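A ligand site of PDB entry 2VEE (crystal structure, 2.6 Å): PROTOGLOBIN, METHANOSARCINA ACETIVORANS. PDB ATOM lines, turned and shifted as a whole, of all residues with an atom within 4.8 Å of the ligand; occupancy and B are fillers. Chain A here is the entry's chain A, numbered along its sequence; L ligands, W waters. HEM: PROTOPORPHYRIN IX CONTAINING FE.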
ATOM      1  N   TYR A   9      12.507  16.477   5.280  1.00  0.00           N
ATOM      2  CA  TYR A   9      11.701  17.669   5.503  1.00  0.00           C
ATOM      3  C   TYR A   9      10.460  17.594   4.610  1.00  0.00           C
ATOM      4  O   TYR A   9      10.565  17.649   3.391  1.00  0.00           O
ATOM      5  CB  TYR A   9      12.513  18.931   5.225  1.00  0.00           C
ATOM      6  CG  TYR A   9      11.721  20.221   5.303  1.00  0.00           C
ATOM      7  CD1 TYR A   9      11.358  20.767   6.544  1.00  0.00           C
ATOM      8  CD2 TYR A   9      11.340  20.898   4.151  1.00  0.00           C
ATOM      9  CE1 TYR A   9      10.627  21.961   6.615  1.00  0.00           C
ATOM     10  CE2 TYR A   9      10.610  22.080   4.211  1.00  0.00           C
ATOM     11  CZ  TYR A   9      10.256  22.610   5.436  1.00  0.00           C
ATOM     12  OH  TYR A   9       9.540  23.783   5.480  1.00  0.00           O
ATOM     13  N   VAL A  64      23.730  21.236  23.562  1.00  0.00           N
ATOM     14  CA  VAL A  64      23.296  19.826  23.597  1.00  0.00           C
ATOM     15  C   VAL A  64      24.465  18.880  23.853  1.00  0.00           C
ATOM     16  O   VAL A  64      24.402  18.016  24.729  1.00  0.00           O
ATOM     17  CB  VAL A  64      22.558  19.399  22.287  1.00  0.00           C
ATOM     18  CG1 VAL A  64      22.153  17.924  22.347  1.00  0.00           C
ATOM     19  CG2 VAL A  64      21.322  20.268  22.046  1.00  0.00           C
ATOM     20  N   LEU A  70      21.460  15.284  27.667  1.00  0.00           N
ATOM     21  CA  LEU A  70      20.745  15.884  26.529  1.00  0.00           C
ATOM     22  C   LEU A  70      21.231  15.309  25.194  1.00  0.00           C
ATOM     23  O   LEU A  70      20.413  14.953  24.338  1.00  0.00           O
ATOM     24  CB  LEU A  70      20.867  17.414  26.543  1.00  0.00           C
ATOM     25  CG  LEU A  70      20.215  18.171  27.695  1.00  0.00           C
ATOM     26  CD1 LEU A  70      20.467  19.669  27.570  1.00  0.00           C
ATOM     27  CD2 LEU A  70      18.711  17.869  27.815  1.00  0.00           C
ATOM     28  N   TYR A  73      19.665  11.910  23.611  1.00  0.00           N
ATOM     29  CA  TYR A  73      18.548  11.748  22.666  1.00  0.00           C
ATOM     30  C   TYR A  73      18.976  11.606  21.199  1.00  0.00           C
ATOM     31  O   TYR A  73      18.145  11.270  20.338  1.00  0.00           O
ATOM     32  CB  TYR A  73      17.523  12.874  22.858  1.00  0.00           C
ATOM     33  CG  TYR A  73      16.889  12.849  24.225  1.00  0.00           C
ATOM     34  CD1 TYR A  73      15.901  11.916  24.540  1.00  0.00           C
ATOM     35  CD2 TYR A  73      17.279  13.746  25.216  1.00  0.00           C
ATOM     36  CE1 TYR A  73      15.318  11.871  25.799  1.00  0.00           C
ATOM     37  CE2 TYR A  73      16.695  13.713  26.488  1.00  0.00           C
ATOM     38  CZ  TYR A  73      15.724  12.770  26.766  1.00  0.00           C
ATOM     39  OH  TYR A  73      15.139  12.726  28.015  1.00  0.00           O
ATOM     40  N   PHE A  74      20.256  11.823  20.921  1.00  0.00           N
ATOM     41  CA  PHE A  74      20.818  11.635  19.582  1.00  0.00           C
ATOM     42  C   PHE A  74      21.762  10.417  19.499  1.00  0.00           C
ATOM     43  O   PHE A  74      22.450  10.246  18.485  1.00  0.00           O
ATOM     44  CB  PHE A  74      21.603  12.891  19.154  1.00  0.00           C
ATOM     45  CG  PHE A  74      20.746  14.044  18.720  1.00  0.00           C
ATOM     46  CD1 PHE A  74      20.333  14.181  17.395  1.00  0.00           C
ATOM     47  CD2 PHE A  74      20.380  15.038  19.631  1.00  0.00           C
ATOM     48  CE1 PHE A  74      19.554  15.275  16.975  1.00  0.00           C
ATOM     49  CE2 PHE A  74      19.611  16.139  19.231  1.00  0.00           C
ATOM     50  CZ  PHE A  74      19.195  16.253  17.904  1.00  0.00           C
ATOM     51  N   TYR A  85      22.752  11.217  12.230  1.00  0.00           N
ATOM     52  CA  TYR A  85      21.487  11.647  12.845  1.00  0.00           C
ATOM     53  C   TYR A  85      21.547  13.120  13.229  1.00  0.00           C
ATOM     54  O   TYR A  85      20.609  13.878  12.954  1.00  0.00           O
ATOM     55  CB  TYR A  85      21.215  10.757  14.067  1.00  0.00           C
ATOM     56  CG  TYR A  85      19.863  10.876  14.772  1.00  0.00           C
ATOM     57  CD1 TYR A  85      18.688  11.206  14.076  1.00  0.00           C
ATOM     58  CD2 TYR A  85      19.761  10.573  16.131  1.00  0.00           C
ATOM     59  CE1 TYR A  85      17.454  11.277  14.747  1.00  0.00           C
ATOM     60  CE2 TYR A  85      18.540  10.648  16.799  1.00  0.00           C
ATOM     61  CZ  TYR A  85      17.392  10.997  16.110  1.00  0.00           C
ATOM     62  OH  TYR A  85      16.195  11.069  16.783  1.00  0.00           O
ATOM     63  N   VAL A  89      19.349  16.110  11.254  1.00  0.00           N
ATOM     64  CA  VAL A  89      18.394  16.912  12.016  1.00  0.00           C
ATOM     65  C   VAL A  89      18.766  18.395  11.955  1.00  0.00           C
ATOM     66  O   VAL A  89      17.882  19.261  11.870  1.00  0.00           O
ATOM     67  CB  VAL A  89      18.231  16.401  13.464  1.00  0.00           C
ATOM     68  CG1 VAL A  89      17.465  17.393  14.343  1.00  0.00           C
ATOM     69  CG2 VAL A  89      17.538  15.043  13.462  1.00  0.00           C
ATOM     70  N   ARG A  92      17.112  20.342   9.073  1.00  0.00           N
ATOM     71  CA  ARG A  92      15.686  20.612   9.298  1.00  0.00           C
ATOM     72  C   ARG A  92      15.461  21.637  10.399  1.00  0.00           C
ATOM     73  O   ARG A  92      14.471  22.368  10.392  1.00  0.00           O
ATOM     74  CB  ARG A  92      14.943  19.320   9.618  1.00  0.00           C
ATOM     75  CG  ARG A  92      14.979  18.316   8.492  1.00  0.00           C
ATOM     76  CD  ARG A  92      13.930  17.257   8.668  1.00  0.00           C
ATOM     77  NE  ARG A  92      14.119  16.485   9.892  1.00  0.00           N
ATOM     78  CZ  ARG A  92      14.836  15.369   9.970  1.00  0.00           C
ATOM     79  NH1 ARG A  92      15.434  14.878   8.900  1.00  0.00           N
ATOM     80  NH2 ARG A  92      14.940  14.731  11.130  1.00  0.00           N
ATOM     81  N   PHE A  93      16.383  21.672  11.361  1.00  0.00           N
ATOM     82  CA  PHE A  93      16.360  22.644  12.438  1.00  0.00           C
ATOM     83  C   PHE A  93      16.662  24.019  11.828  1.00  0.00           C
ATOM     84  O   PHE A  93      15.983  25.005  12.117  1.00  0.00           O
ATOM     85  CB  PHE A  93      17.454  22.282  13.438  1.00  0.00           C
ATOM     86  CG  PHE A  93      17.085  22.516  14.874  1.00  0.00           C
ATOM     87  CD1 PHE A  93      16.691  23.773  15.311  1.00  0.00           C
ATOM     88  CD2 PHE A  93      17.159  21.475  15.796  1.00  0.00           C
ATOM     89  CE1 PHE A  93      16.351  23.990  16.644  1.00  0.00           C
ATOM     90  CE2 PHE A  93      16.838  21.680  17.134  1.00  0.00           C
ATOM     91  CZ  PHE A  93      16.434  22.944  17.564  1.00  0.00           C
ATOM     92  N   TRP A  96      13.868  25.253  10.001  1.00  0.00           N
ATOM     93  CA  TRP A  96      12.768  25.616  10.879  1.00  0.00           C
ATOM     94  C   TRP A  96      12.840  27.058  11.359  1.00  0.00           C
ATOM     95  O   TRP A  96      11.810  27.696  11.555  1.00  0.00           O
ATOM     96  CB  TRP A  96      12.695  24.653  12.065  1.00  0.00           C
ATOM     97  CG  TRP A  96      11.854  25.128  13.199  1.00  0.00           C
ATOM     98  CD1 TRP A  96      10.511  24.973  13.354  1.00  0.00           C
ATOM     99  CD2 TRP A  96      12.316  25.816  14.361  1.00  0.00           C
ATOM    100  NE1 TRP A  96      10.097  25.527  14.536  1.00  0.00           N
ATOM    101  CE2 TRP A  96      11.186  26.058  15.187  1.00  0.00           C
ATOM    102  CE3 TRP A  96      13.569  26.271  14.798  1.00  0.00           C
ATOM    103  CZ2 TRP A  96      11.274  26.717  16.412  1.00  0.00           C
ATOM    104  CZ3 TRP A  96      13.666  26.924  16.020  1.00  0.00           C
ATOM    105  CH2 TRP A  96      12.516  27.154  16.807  1.00  0.00           C
ATOM    106  N   TYR A 112       2.336  20.645  10.015  1.00  0.00           N
ATOM    107  CA  TYR A 112       3.736  20.344  10.299  1.00  0.00           C
ATOM    108  C   TYR A 112       4.090  20.407  11.781  1.00  0.00           C
ATOM    109  O   TYR A 112       4.996  19.703  12.236  1.00  0.00           O
ATOM    110  CB  TYR A 112       4.685  21.219   9.478  1.00  0.00           C
ATOM    111  CG  TYR A 112       6.021  20.547   9.206  1.00  0.00           C
ATOM    112  CD1 TYR A 112       6.070  19.300   8.581  1.00  0.00           C
ATOM    113  CD2 TYR A 112       7.221  21.150   9.573  1.00  0.00           C
ATOM    114  CE1 TYR A 112       7.292  18.674   8.321  1.00  0.00           C
ATOM    115  CE2 TYR A 112       8.443  20.524   9.313  1.00  0.00           C
ATOM    116  CZ  TYR A 112       8.466  19.294   8.686  1.00  0.00           C
ATOM    117  OH  TYR A 112       9.666  18.669   8.431  1.00  0.00           O
ATOM    118  N   ILE A 116       6.042  17.718  13.741  1.00  0.00           N
ATOM    119  CA  ILE A 116       7.221  17.960  14.579  1.00  0.00           C
ATOM    120  C   ILE A 116       7.033  17.405  15.995  1.00  0.00           C
ATOM    121  O   ILE A 116       7.951  16.787  16.554  1.00  0.00           O
ATOM    122  CB  ILE A 116       7.675  19.451  14.604  1.00  0.00           C
ATOM    123  CG1 ILE A 116       8.065  19.918  13.191  1.00  0.00           C
ATOM    124  CG2 ILE A 116       8.860  19.642  15.558  1.00  0.00           C
ATOM    125  CD1 ILE A 116       8.463  21.385  13.090  1.00  0.00           C
ATOM    126  N   ARG A 119       7.500  13.586  15.880  1.00  0.00           N
ATOM    127  CA  ARG A 119       8.890  13.162  15.682  1.00  0.00           C
ATOM    128  C   ARG A 119       9.743  13.297  16.954  1.00  0.00           C
ATOM    129  O   ARG A 119      10.785  12.663  17.057  1.00  0.00           O
ATOM    130  CB  ARG A 119       9.532  13.943  14.535  1.00  0.00           C
ATOM    131  CG  ARG A 119       8.898  13.722  13.159  1.00  0.00           C
ATOM    132  CD  ARG A 119       9.632  14.576  12.125  1.00  0.00           C
ATOM    133  NE  ARG A 119       9.028  14.501  10.793  1.00  0.00           N
ATOM    134  CZ  ARG A 119       9.630  14.885   9.671  1.00  0.00           C
ATOM    135  NH1 ARG A 119      10.876  15.368   9.689  1.00  0.00           N
ATOM    136  NH2 ARG A 119       8.999  14.779   8.507  1.00  0.00           N
ATOM    137  N   HIS A 120       9.325  14.158  17.880  1.00  0.00           N
ATOM    138  CA  HIS A 120      10.001  14.272  19.169  1.00  0.00           C
ATOM    139  C   HIS A 120       9.544  13.144  20.078  1.00  0.00           C
ATOM    140  O   HIS A 120      10.282  12.682  20.950  1.00  0.00           O
ATOM    141  CB  HIS A 120       9.680  15.614  19.829  1.00  0.00           C
ATOM    142  CG  HIS A 120      10.529  16.749  19.338  1.00  0.00           C
ATOM    143  ND1 HIS A 120      10.274  17.397  18.142  1.00  0.00           N
ATOM    144  CD2 HIS A 120      11.623  17.335  19.862  1.00  0.00           C
ATOM    145  CE1 HIS A 120      11.180  18.344  17.963  1.00  0.00           C
ATOM    146  NE2 HIS A 120      12.018  18.324  18.989  1.00  0.00           N
ATOM    147  N   LYS A 124       6.746   8.882  16.202  1.00  0.00           N
ATOM    148  CA  LYS A 124       7.548   8.969  14.981  1.00  0.00           C
ATOM    149  C   LYS A 124       9.050   9.237  15.146  1.00  0.00           C
ATOM    150  O   LYS A 124       9.771   9.292  14.147  1.00  0.00           O
ATOM    151  CB  LYS A 124       6.930   9.955  13.980  1.00  0.00           C
ATOM    152  CG  LYS A 124       5.717   9.430  13.234  1.00  0.00           C
ATOM    153  CD  LYS A 124       5.372  10.286  12.006  1.00  0.00           C
ATOM    154  CE  LYS A 124       6.137   9.822  10.766  1.00  0.00           C
ATOM    155  NZ  LYS A 124       5.994  10.800   9.633  1.00  0.00           N
ATOM    156  N   LYS A 125       9.530   9.400  16.375  1.00  0.00           N
ATOM    157  CA  LYS A 125      10.976   9.621  16.609  1.00  0.00           C
ATOM    158  C   LYS A 125      11.833   8.491  16.051  1.00  0.00           C
ATOM    159  O   LYS A 125      11.539   7.312  16.272  1.00  0.00           O
ATOM    160  CB  LYS A 125      11.301   9.807  18.104  1.00  0.00           C
ATOM    161  CG  LYS A 125      12.756  10.221  18.343  1.00  0.00           C
ATOM    162  CD  LYS A 125      13.097  10.304  19.820  1.00  0.00           C
ATOM    163  CE  LYS A 125      14.498  10.880  20.032  1.00  0.00           C
ATOM    164  NZ  LYS A 125      15.604   9.879  19.891  1.00  0.00           N
ATOM    165  N   ASN A 126      12.905   8.858  15.325  1.00  0.00           N
ATOM    166  CA  ASN A 126      13.826   7.901  14.715  1.00  0.00           C
ATOM    167  C   ASN A 126      13.416   7.344  13.352  1.00  0.00           C
ATOM    168  O   ASN A 126      14.212   6.674  12.677  1.00  0.00           O
ATOM    169  CB  ASN A 126      14.060   6.680  15.605  1.00  0.00           C
ATOM    170  CG  ASN A 126      14.602   7.039  16.961  1.00  0.00           C
ATOM    171  OD1 ASN A 126      15.557   7.816  17.067  1.00  0.00           O
ATOM    172  ND2 ASN A 126      14.003   6.501  18.008  1.00  0.00           N
ATOM    173  N   THR A 128      12.001   9.274  10.567  1.00  0.00           N
ATOM    174  CA  THR A 128      12.368  10.188   9.483  1.00  0.00           C
ATOM    175  C   THR A 128      13.787   9.957   8.933  1.00  0.00           C
ATOM    176  O   THR A 128      13.985   9.885   7.716  1.00  0.00           O
ATOM    177  CB  THR A 128      12.179  11.648   9.911  1.00  0.00           C
ATOM    178  OG1 THR A 128      10.803  11.865  10.242  1.00  0.00           O
ATOM    179  CG2 THR A 128      12.573  12.604   8.795  1.00  0.00           C
ATOM    180  N   ASP A 129      14.767   9.828   9.816  1.00  0.00           N
ATOM    181  CA  ASP A 129      16.132   9.607   9.384  1.00  0.00           C
ATOM    182  C   ASP A 129      16.510   8.136   9.418  1.00  0.00           C
ATOM    183  O   ASP A 129      17.647   7.772   9.111  1.00  0.00           O
ATOM    184  CB  ASP A 129      17.099  10.433  10.231  1.00  0.00           C
ATOM    185  CG  ASP A 129      16.798  11.893  10.157  1.00  0.00           C
ATOM    186  OD1 ASP A 129      16.862  12.464   9.042  1.00  0.00           O
ATOM    187  OD2 ASP A 129      16.476  12.486  11.208  1.00  0.00           O
ATOM    188  N   ILE A 137      11.734  11.421  23.490  1.00  0.00           N
ATOM    189  CA  ILE A 137      12.257  12.577  24.217  1.00  0.00           C
ATOM    190  C   ILE A 137      11.191  13.014  25.212  1.00  0.00           C
ATOM    191  O   ILE A 137      10.100  13.408  24.807  1.00  0.00           O
ATOM    192  CB  ILE A 137      12.619  13.774  23.299  1.00  0.00           C
ATOM    193  CG1 ILE A 137      13.421  13.323  22.073  1.00  0.00           C
ATOM    194  CG2 ILE A 137      13.392  14.836  24.079  1.00  0.00           C
ATOM    195  CD1 ILE A 137      13.437  14.345  20.940  1.00  0.00           C
ATOM    196  N   TYR A 141      11.767  18.172  28.780  1.00  0.00           N
ATOM    197  CA  TYR A 141      12.901  18.817  28.142  1.00  0.00           C
ATOM    198  C   TYR A 141      12.489  19.701  26.954  1.00  0.00           C
ATOM    199  O   TYR A 141      13.157  20.688  26.670  1.00  0.00           O
ATOM    200  CB  TYR A 141      14.018  17.810  27.779  1.00  0.00           C
ATOM    201  CG  TYR A 141      14.667  17.179  29.000  1.00  0.00           C
ATOM    202  CD1 TYR A 141      15.356  17.965  29.926  1.00  0.00           C
ATOM    203  CD2 TYR A 141      14.576  15.806  29.239  1.00  0.00           C
ATOM    204  CE1 TYR A 141      15.933  17.401  31.059  1.00  0.00           C
ATOM    205  CE2 TYR A 141      15.148  15.234  30.372  1.00  0.00           C
ATOM    206  CZ  TYR A 141      15.829  16.036  31.282  1.00  0.00           C
ATOM    207  OH  TYR A 141      16.410  15.482  32.405  1.00  0.00           O
ATOM    208  N   LEU A 142      11.387  19.354  26.290  1.00  0.00           N
ATOM    209  CA  LEU A 142      10.822  20.238  25.273  1.00  0.00           C
ATOM    210  C   LEU A 142      10.403  21.581  25.884  1.00  0.00           C
ATOM    211  O   LEU A 142      10.650  22.637  25.293  1.00  0.00           O
ATOM    212  CB  LEU A 142       9.643  19.575  24.551  1.00  0.00           C
ATOM    213  CG  LEU A 142       9.897  18.743  23.284  1.00  0.00           C
ATOM    214  CD1 LEU A 142      10.819  17.550  23.542  1.00  0.00           C
ATOM    215  CD2 LEU A 142       8.589  18.287  22.642  1.00  0.00           C
ATOM    216  N   PHE A 145      13.488  23.612  27.042  1.00  0.00           N
ATOM    217  CA  PHE A 145      14.189  24.205  25.906  1.00  0.00           C
ATOM    218  C   PHE A 145      13.602  25.534  25.414  1.00  0.00           C
ATOM    219  O   PHE A 145      14.246  26.255  24.652  1.00  0.00           O
ATOM    220  CB  PHE A 145      14.331  23.207  24.756  1.00  0.00           C
ATOM    221  CG  PHE A 145      15.618  22.412  24.789  1.00  0.00           C
ATOM    222  CD1 PHE A 145      16.155  21.967  25.989  1.00  0.00           C
ATOM    223  CD2 PHE A 145      16.273  22.097  23.607  1.00  0.00           C
ATOM    224  CE1 PHE A 145      17.337  21.224  26.013  1.00  0.00           C
ATOM    225  CE2 PHE A 145      17.450  21.357  23.611  1.00  0.00           C
ATOM    226  CZ  PHE A 145      17.982  20.915  24.823  1.00  0.00           C
ATOM    227  N   ILE A 146      12.387  25.875  25.859  1.00  0.00           N
ATOM    228  CA  ILE A 146      11.855  27.206  25.572  1.00  0.00           C
ATOM    229  C   ILE A 146      12.881  28.255  25.991  1.00  0.00           C
ATOM    230  O   ILE A 146      13.160  29.174  25.228  1.00  0.00           O
ATOM    231  CB  ILE A 146      10.471  27.462  26.221  1.00  0.00           C
ATOM    232  CG1 ILE A 146       9.417  26.594  25.523  1.00  0.00           C
ATOM    233  CG2 ILE A 146      10.078  28.930  26.108  1.00  0.00           C
ATOM    234  CD1 ILE A 146       8.151  26.380  26.337  1.00  0.00           C
ATOM    235  N   ILE A 149      16.404  28.127  23.743  1.00  0.00           N
ATOM    236  CA  ILE A 149      16.025  28.430  22.361  1.00  0.00           C
ATOM    237  C   ILE A 149      15.555  29.875  22.201  1.00  0.00           C
ATOM    238  O   ILE A 149      15.784  30.487  21.146  1.00  0.00           O
ATOM    239  CB  ILE A 149      14.962  27.439  21.793  1.00  0.00           C
ATOM    240  CG1 ILE A 149      15.524  26.008  21.717  1.00  0.00           C
ATOM    241  CG2 ILE A 149      14.446  27.907  20.426  1.00  0.00           C
ATOM    242  CD1 ILE A 149      16.644  25.797  20.690  1.00  0.00           C
ATOM    243  N   THR A 178       8.300  30.453  19.659  1.00  0.00           N
ATOM    244  CA  THR A 178       8.900  29.268  20.262  1.00  0.00           C
ATOM    245  C   THR A 178       7.939  28.681  21.294  1.00  0.00           C
ATOM    246  O   THR A 178       7.660  27.481  21.260  1.00  0.00           O
ATOM    247  CB  THR A 178      10.264  29.584  20.892  1.00  0.00           C
ATOM    248  OG1 THR A 178      11.118  30.155  19.894  1.00  0.00           O
ATOM    249  CG2 THR A 178      10.914  28.310  21.440  1.00  0.00           C
ATOM    250  N   VAL A 182       6.140  24.883  20.952  1.00  0.00           N
ATOM    251  CA  VAL A 182       6.319  23.883  22.011  1.00  0.00           C
ATOM    252  C   VAL A 182       4.954  23.484  22.562  1.00  0.00           C
ATOM    253  O   VAL A 182       4.684  22.290  22.734  1.00  0.00           O
ATOM    254  CB  VAL A 182       7.255  24.366  23.148  1.00  0.00           C
ATOM    255  CG1 VAL A 182       7.244  23.376  24.315  1.00  0.00           C
ATOM    256  CG2 VAL A 182       8.676  24.544  22.625  1.00  0.00           C
ATOM    257  N   TRP A 185       3.335  21.183  20.205  1.00  0.00           N
ATOM    258  CA  TRP A 185       4.096  19.924  20.159  1.00  0.00           C
ATOM    259  C   TRP A 185       3.785  18.976  21.329  1.00  0.00           C
ATOM    260  O   TRP A 185       4.215  17.825  21.334  1.00  0.00           O
ATOM    261  CB  TRP A 185       5.610  20.162  20.079  1.00  0.00           C
ATOM    262  CG  TRP A 185       6.063  20.941  18.872  1.00  0.00           C
ATOM    263  CD1 TRP A 185       5.314  21.246  17.773  1.00  0.00           C
ATOM    264  CD2 TRP A 185       7.364  21.484  18.647  1.00  0.00           C
ATOM    265  NE1 TRP A 185       6.072  21.969  16.871  1.00  0.00           N
ATOM    266  CE2 TRP A 185       7.329  22.128  17.389  1.00  0.00           C
ATOM    267  CE3 TRP A 185       8.554  21.497  19.388  1.00  0.00           C
ATOM    268  CZ2 TRP A 185       8.445  22.772  16.848  1.00  0.00           C
ATOM    269  CZ3 TRP A 185       9.657  22.137  18.849  1.00  0.00           C
ATOM    270  CH2 TRP A 185       9.601  22.770  17.584  1.00  0.00           C
HETATM  271  CHA HEM L   1      13.988  17.575  15.873  1.00  0.00           C
HETATM  272  CHB HEM L   1      13.293  22.140  17.351  1.00  0.00           C
HETATM  273  CHC HEM L   1      13.343  20.499  21.883  1.00  0.00           C
HETATM  274  CHD HEM L   1      16.207  16.968  20.173  1.00  0.00           C
HETATM  275  C1A HEM L   1      13.687  18.917  15.834  1.00  0.00           C
HETATM  276  C2A HEM L   1      13.264  19.702  14.687  1.00  0.00           C
HETATM  277  C3A HEM L   1      13.075  20.964  15.108  1.00  0.00           C
HETATM  278  C4A HEM L   1      13.373  21.027  16.530  1.00  0.00           C
HETATM  279  CMA HEM L   1      12.624  22.141  14.231  1.00  0.00           C
HETATM  280  CAA HEM L   1      13.070  19.191  13.229  1.00  0.00           C
HETATM  281  CBA HEM L   1      11.627  18.816  12.920  1.00  0.00           C
HETATM  282  CGA HEM L   1      11.589  18.303  11.497  1.00  0.00           C
HETATM  283  O1A HEM L   1      11.294  19.104  10.571  1.00  0.00           O
HETATM  284  O2A HEM L   1      11.858  17.098  11.294  1.00  0.00           O
HETATM  285  C1B HEM L   1      13.164  22.123  18.726  1.00  0.00           C
HETATM  286  C2B HEM L   1      12.717  23.201  19.606  1.00  0.00           C
HETATM  287  C3B HEM L   1      12.725  22.750  20.866  1.00  0.00           C
HETATM  288  C4B HEM L   1      13.180  21.361  20.832  1.00  0.00           C
HETATM  289  CMB HEM L   1      12.302  24.613  19.148  1.00  0.00           C
HETATM  290  CAB HEM L   1      12.327  23.517  22.147  1.00  0.00           C
HETATM  291  CBB HEM L   1      12.282  24.855  22.234  1.00  0.00           C
HETATM  292  C1C HEM L   1      14.228  19.434  21.857  1.00  0.00           C
HETATM  293  C2C HEM L   1      14.851  18.749  22.982  1.00  0.00           C
HETATM  294  C3C HEM L   1      15.640  17.778  22.515  1.00  0.00           C
HETATM  295  C4C HEM L   1      15.558  17.807  21.066  1.00  0.00           C
HETATM  296  CMC HEM L   1      14.641  19.074  24.477  1.00  0.00           C
HETATM  297  CAC HEM L   1      16.498  16.810  23.359  1.00  0.00           C
HETATM  298  CBC HEM L   1      17.704  17.188  23.795  1.00  0.00           C
HETATM  299  C1D HEM L   1      15.742  16.644  18.919  1.00  0.00           C
HETATM  300  C2D HEM L   1      15.853  15.371  18.234  1.00  0.00           C
HETATM  301  C3D HEM L   1      15.156  15.575  16.881  1.00  0.00           C
HETATM  302  C4D HEM L   1      14.679  16.942  16.886  1.00  0.00           C
HETATM  303  CMD HEM L   1      16.551  14.080  18.737  1.00  0.00           C
HETATM  304  CAD HEM L   1      14.990  14.531  15.765  1.00  0.00           C
HETATM  305  CBD HEM L   1      13.799  13.663  16.156  1.00  0.00           C
HETATM  306  CGD HEM L   1      13.477  12.666  15.073  1.00  0.00           C
HETATM  307  O1D HEM L   1      12.615  12.993  14.221  1.00  0.00           O
HETATM  308  O2D HEM L   1      14.067  11.558  15.078  1.00  0.00           O
HETATM  309  NA  HEM L   1      13.738  19.762  16.928  1.00  0.00           N
HETATM  310  NB  HEM L   1      13.427  21.025  19.513  1.00  0.00           N
HETATM  311  NC  HEM L   1      14.697  18.811  20.715  1.00  0.00           N
HETATM  312  ND  HEM L   1      15.045  17.526  18.098  1.00  0.00           N
HETATM  313 FE   HEM L   1      14.085  19.150  18.874  1.00  0.00          FE
HETATM  314  O   HOH W   1      13.231  15.604  13.041  1.00  0.00           O
HETATM  315  O   HOH W   2      11.709  21.591  10.478  1.00  0.00           O
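Water W2 lies within hydrogen-bond range of O1A of the ligand (2.5 Å) and O of Arg 92 (2.9 Å). Water W1 bridges an oxygen (O2A) of the ligand (2.7 Å) and the guanidinium group (NH2) of Arg 92 (2.7 Å).
The side-chain amide oxygen of Asn 126 lies within hydrogen-bond range of the side-chain hydroxyl of Tyr 85 (3.3 Å). The guanidinium group (NH2) of Arg 92 lies within salt-bridge range of the side-chain carboxylate (OD2) of Asp 129. The side-chain hydroxyl of Thr 128 lies within hydrogen-bond range of the guanidinium group of Arg 119. The side-chain amino group (NZ) of Lys 125 sits at hydrogen-bond distance from the side-chain amide oxygen (OD1) of Asn 126. The side-chain hydroxyl (OH) of Tyr 85 lies within hydrogen-bond range of the side-chain amino group (NZ) of Lys 125, 3.4 Å away. A ring nitrogen (ND1) of His 120 is in hydrogen-bond range of the backbone carbonyl oxygen (O) of Ile 116, 2.9 Å away. The backbone carbonyl oxygen (O) of Tyr 73 is in hydrogen-bond range of the side-chain amino group (NZ) of Lys 125. The backbone carbonyl oxygen (O) of His 120 is in hydrogen-bond range of the backbone NH (N) of Ile 137 (3.2 Å).
Leu 70 touches the ligand. O of Tyr 73 touches CMD of the ligand, at 3.6 Å. Phe 74 touches the ligand. Val 89 touches the ligand. CZ of Phe 93 touches CHB of the ligand (3.2 Å). Trp 96 touches the ligand (CG to CMA, 3.3 Å). Ile 116 touches the ligand (CG1 to CBA, 3.7 Å). Lys 125 touches the ligand (CG to O2D, 3.8 Å). Ile 137 touches the ligand (CG2 to CAC, 3.7 Å). Tyr 141 touches the ligand. O of Leu 142 touches CAB of the ligand, 3.7 Å away. Phe 145 touches the ligand (CB to CAB, 3.3 Å). Ile 146 touches the ligand. CG1 of Ile 149 touches CBB of the ligand, at 3.5 Å. Thr 178 touches the ligand (CG2 to CBB, 3.8 Å). Val 182 touches the ligand (CG2 to CBB, 3.6 Å). CZ3 of Trp 185 touches C2B of the ligand, at 3.3 Å. Hydrophobic or aromatic side chains within 4 Å of the ligand: Tyr 73, Phe 74, Tyr 85, Val 89, Phe 93, Trp 96, Tyr 112, Ile 116, His 120, Ile 137, Tyr 141, Phe 145, Ile 149, Val 182 and Trp 185. 23 residues have an atom within 4 Å of the ligand: Leu 70, Tyr 73, Phe 74, Tyr 85, Val 89, Arg 92, Phe 93, Trp 96, Tyr 112, Ile 116, Arg 119, His 120, Lys 125, Asn 126, Ile 137, Tyr 141, Leu 142, Phe 145, Ile 146, Ile 149, Thr 178, Val 182 and Trp 185. The nearest printed residue that does not touch the ligand is Tyr 9 (4.4 Å).
N of Asn 126 sits at hydrogen-bond distance from O2D of the ligand, at 2.9 Å. An oxygen (O2D) of the ligand is in hydrogen-bond range of the side-chain hydroxyl (OH) of Tyr 85 (2.8 Å). NE2 of His 120 is bound to FE of the ligand (2.2 Å). NE of Arg 92 is in salt-bridge range of O2A of the ligand, at 2.7 Å. An oxygen (O1A) of the ligand is in hydrogen-bond range of the side-chain hydroxyl of Tyr 112 (2.7 Å). An oxygen (O2A) of the ligand is in salt-bridge range of the guanidinium group of Arg 119 (2.6 Å).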
